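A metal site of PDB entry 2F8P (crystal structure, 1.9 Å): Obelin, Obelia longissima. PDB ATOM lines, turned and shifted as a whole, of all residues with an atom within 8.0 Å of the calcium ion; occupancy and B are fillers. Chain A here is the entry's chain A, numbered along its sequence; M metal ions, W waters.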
ATOM      1  N   PHE A  26     -35.238  17.098   4.605  1.00  0.00           N
ATOM      2  CA  PHE A  26     -34.041  16.659   5.325  1.00  0.00           C
ATOM      3  C   PHE A  26     -32.778  17.201   4.641  1.00  0.00           C
ATOM      4  O   PHE A  26     -31.928  17.844   5.306  1.00  0.00           O
ATOM      5  CB  PHE A  26     -34.028  15.110   5.422  1.00  0.00           C
ATOM      6  CG  PHE A  26     -32.838  14.529   6.126  1.00  0.00           C
ATOM      7  CD1 PHE A  26     -32.899  14.173   7.465  1.00  0.00           C
ATOM      8  CD2 PHE A  26     -31.635  14.315   5.421  1.00  0.00           C
ATOM      9  CE1 PHE A  26     -31.787  13.608   8.128  1.00  0.00           C
ATOM     10  CE2 PHE A  26     -30.525  13.791   6.064  1.00  0.00           C
ATOM     11  CZ  PHE A  26     -30.591  13.426   7.425  1.00  0.00           C
ATOM     12  N   LEU A  29     -32.591  21.040   4.890  1.00  0.00           N
ATOM     13  CA  LEU A  29     -32.241  21.462   6.243  1.00  0.00           C
ATOM     14  C   LEU A  29     -30.826  21.030   6.717  1.00  0.00           C
ATOM     15  O   LEU A  29     -30.301  21.579   7.706  1.00  0.00           O
ATOM     16  CB  LEU A  29     -33.281  20.980   7.252  1.00  0.00           C
ATOM     17  CG  LEU A  29     -34.733  21.456   7.010  1.00  0.00           C
ATOM     18  CD1 LEU A  29     -35.685  20.695   7.893  1.00  0.00           C
ATOM     19  CD2 LEU A  29     -34.858  22.925   7.237  1.00  0.00           C
ATOM     20  N   ASP A  30     -30.216  20.067   6.021  1.00  0.00           N
ATOM     21  CA  ASP A  30     -28.895  19.552   6.390  1.00  0.00           C
ATOM     22  C   ASP A  30     -27.837  20.544   5.931  1.00  0.00           C
ATOM     23  O   ASP A  30     -27.226  20.383   4.850  1.00  0.00           O
ATOM     24  CB  ASP A  30     -28.676  18.177   5.764  1.00  0.00           C
ATOM     25  CG  ASP A  30     -27.292  17.574   6.067  1.00  0.00           C
ATOM     26  OD1 ASP A  30     -26.587  17.949   7.044  1.00  0.00           O
ATOM     27  OD2 ASP A  30     -26.949  16.649   5.289  1.00  0.00           O
ATOM     28  N   ILE A  31     -27.633  21.562   6.744  1.00  0.00           N
ATOM     29  CA  ILE A  31     -26.809  22.711   6.373  1.00  0.00           C
ATOM     30  C   ILE A  31     -25.370  22.295   5.926  1.00  0.00           C
ATOM     31  O   ILE A  31     -24.931  22.696   4.857  1.00  0.00           O
ATOM     32  CB  ILE A  31     -26.741  23.766   7.489  1.00  0.00           C
ATOM     33  CG1 ILE A  31     -28.140  24.365   7.788  1.00  0.00           C
ATOM     34  CG2 ILE A  31     -25.788  24.886   7.098  1.00  0.00           C
ATOM     35  CD1 ILE A  31     -28.131  25.292   9.007  1.00  0.00           C
ATOM     36  N   ASN A  32     -24.687  21.503   6.735  1.00  0.00           N
ATOM     37  CA  ASN A  32     -23.281  21.149   6.448  1.00  0.00           C
ATOM     38  C   ASN A  32     -23.165  19.913   5.528  1.00  0.00           C
ATOM     39  O   ASN A  32     -22.052  19.470   5.212  1.00  0.00           O
ATOM     40  CB  ASN A  32     -22.515  20.943   7.752  1.00  0.00           C
ATOM     41  CG  ASN A  32     -22.923  19.687   8.455  1.00  0.00           C
ATOM     42  OD1 ASN A  32     -23.848  19.024   8.021  1.00  0.00           O
ATOM     43  ND2 ASN A  32     -22.239  19.351   9.549  1.00  0.00           N
ATOM     44  N   GLY A  33     -24.305  19.351   5.119  1.00  0.00           N
ATOM     45  CA  GLY A  33     -24.348  18.383   4.029  1.00  0.00           C
ATOM     46  C   GLY A  33     -23.747  17.024   4.329  1.00  0.00           C
ATOM     47  O   GLY A  33     -23.400  16.280   3.403  1.00  0.00           O
ATOM     48  N   ASN A  34     -23.659  16.684   5.616  1.00  0.00           N
ATOM     49  CA  ASN A  34     -23.017  15.441   6.055  1.00  0.00           C
ATOM     50  C   ASN A  34     -23.993  14.248   6.131  1.00  0.00           C
ATOM     51  O   ASN A  34     -23.624  13.180   6.593  1.00  0.00           O
ATOM     52  CB  ASN A  34     -22.270  15.640   7.387  1.00  0.00           C
ATOM     53  CG  ASN A  34     -23.208  15.826   8.579  1.00  0.00           C
ATOM     54  OD1 ASN A  34     -24.394  16.142   8.438  1.00  0.00           O
ATOM     55  ND2 ASN A  34     -22.662  15.627   9.777  1.00  0.00           N
ATOM     56  N   GLY A  35     -25.227  14.434   5.658  1.00  0.00           N
ATOM     57  CA  GLY A  35     -26.259  13.386   5.698  1.00  0.00           C
ATOM     58  C   GLY A  35     -26.809  13.068   7.066  1.00  0.00           C
ATOM     59  O   GLY A  35     -27.384  11.992   7.272  1.00  0.00           O
ATOM     60  N   LYS A  36     -26.576  13.949   8.028  1.00  0.00           N
ATOM     61  CA  LYS A  36     -27.216  13.824   9.318  1.00  0.00           C
ATOM     62  C   LYS A  36     -27.825  15.190   9.684  1.00  0.00           C
ATOM     63  O   LYS A  36     -27.269  16.225   9.328  1.00  0.00           O
ATOM     64  CB  LYS A  36     -26.248  13.333  10.415  1.00  0.00           C
ATOM     65  CG  LYS A  36     -25.615  11.893  10.209  1.00  0.00           C
ATOM     66  CD  LYS A  36     -25.719  11.074  11.502  1.00  0.00           C
ATOM     67  CE  LYS A  36     -25.130   9.677  11.392  1.00  0.00           C
ATOM     68  NZ  LYS A  36     -23.754   9.723  10.803  1.00  0.00           N
ATOM     69  N   ILE A  37     -28.966  15.175  10.370  1.00  0.00           N
ATOM     70  CA  ILE A  37     -29.688  16.391  10.712  1.00  0.00           C
ATOM     71  C   ILE A  37     -29.583  16.595  12.233  1.00  0.00           C
ATOM     72  O   ILE A  37     -29.671  15.637  12.972  1.00  0.00           O
ATOM     73  CB  ILE A  37     -31.176  16.295  10.219  1.00  0.00           C
ATOM     74  CG1 ILE A  37     -31.855  17.647  10.195  1.00  0.00           C
ATOM     75  CG2 ILE A  37     -31.988  15.255  11.023  1.00  0.00           C
ATOM     76  CD1 ILE A  37     -31.204  18.608   9.277  1.00  0.00           C
ATOM     77  N   THR A  38     -29.366  17.828  12.695  1.00  0.00           N
ATOM     78  CA  THR A  38     -29.434  18.131  14.124  1.00  0.00           C
ATOM     79  C   THR A  38     -30.580  19.133  14.374  1.00  0.00           C
ATOM     80  O   THR A  38     -31.023  19.807  13.462  1.00  0.00           O
ATOM     81  CB  THR A  38     -28.138  18.803  14.627  1.00  0.00           C
ATOM     82  OG1 THR A  38     -27.957  20.018  13.905  1.00  0.00           O
ATOM     83  CG2 THR A  38     -26.910  17.896  14.413  1.00  0.00           C
ATOM     84  N   GLU A  41     -29.462  22.576  13.175  1.00  0.00           N
ATOM     85  CA  GLU A  41     -29.658  22.887  11.750  1.00  0.00           C
ATOM     86  C   GLU A  41     -31.116  23.188  11.426  1.00  0.00           C
ATOM     87  O   GLU A  41     -31.423  24.154  10.732  1.00  0.00           O
ATOM     88  CB  GLU A  41     -29.172  21.703  10.915  1.00  0.00           C
ATOM     89  CG  GLU A  41     -27.658  21.596  10.872  1.00  0.00           C
ATOM     90  CD  GLU A  41     -27.177  20.415  10.081  1.00  0.00           C
ATOM     91  OE1 GLU A  41     -27.841  19.335  10.111  1.00  0.00           O
ATOM     92  OE2 GLU A  41     -26.089  20.534   9.415  1.00  0.00           O
ATOM     93  N   GLU A  82     -26.957  14.090  16.179  1.00  0.00           N
ATOM     94  CA  GLU A  82     -26.938  13.870  14.741  1.00  0.00           C
ATOM     95  C   GLU A  82     -27.757  12.642  14.372  1.00  0.00           C
ATOM     96  O   GLU A  82     -27.495  11.548  14.878  1.00  0.00           O
ATOM     97  CB  GLU A  82     -25.512  13.721  14.216  1.00  0.00           C
ATOM     98  CG  GLU A  82     -24.669  14.972  14.428  1.00  0.00           C
ATOM     99  CD  GLU A  82     -23.671  15.132  13.326  1.00  0.00           C
ATOM    100  OE1 GLU A  82     -22.607  14.464  13.411  1.00  0.00           O
ATOM    101  OE2 GLU A  82     -23.957  15.884  12.370  1.00  0.00           O
ATOM    102  N   ILE A  83     -28.740  12.823  13.473  1.00  0.00           N
ATOM    103  CA  ILE A  83     -29.749  11.783  13.191  1.00  0.00           C
ATOM    104  C   ILE A  83     -29.811  11.559  11.690  1.00  0.00           C
ATOM    105  O   ILE A  83     -29.997  12.508  10.956  1.00  0.00           O
ATOM    106  CB  ILE A  83     -31.199  12.163  13.733  1.00  0.00           C
ATOM    107  CG1 ILE A  83     -31.221  12.407  15.274  1.00  0.00           C
ATOM    108  CG2 ILE A  83     -32.234  11.096  13.356  1.00  0.00           C
ATOM    109  CD1 ILE A  83     -30.569  11.314  16.089  1.00  0.00           C
HETATM  110 CA    CA M   1     -25.897  17.991   9.026  1.00  0.00          CA
HETATM  111  O   HOH W   1     -24.966  17.909  11.123  1.00  0.00           O
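The side-chain carboxylate (OD1) of Asp 30 is bound to the calcium ion, at 2.1 Å. O of Lys 36 binds the calcium ion (2.3 Å). Water W1 is bound to the calcium ion (2.3 Å). The side-chain amide oxygen (OD1) of Asn 34 binds the calcium ion. The calcium ion is bound by the side-chain amide oxygen (OD1) of Asn 32 (2.5 Å). The calcium ion is bound by OE2 of Glu 41, at 2.6 Å. OE1 of Glu 41 is bound to the calcium ion (2.6 Å). The calcium ion has seven donor atoms within binding distance.
The side-chain carboxylate of Asp 30 lies close to the backbone NH of Gly 33, at 3.3 Å. The side-chain carboxylate (OD2) of Asp 30 lies within hydrogen-bond range of the backbone NH (N) of Gly 35 (2.8 Å). ND2 of Asn 34 sits at hydrogen-bond distance from OE2 of Glu 82 (2.9 Å). OE2 of Glu 41 lies close to N of Ile 31 (3.3 Å). The backbone NH of Glu 41 lies within hydrogen-bond range of the side-chain hydroxyl of Thr 38 (3.1 Å).
Water W1 bridges the side-chain carboxylate of Glu 82 (2.6 Å) and the side-chain amide nitrogen of Asn 32 (3.5 Å).
Within 4 Å of the calcium ion: Asp 30, Asn 32, Asn 34, Lys 36 and Glu 41.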
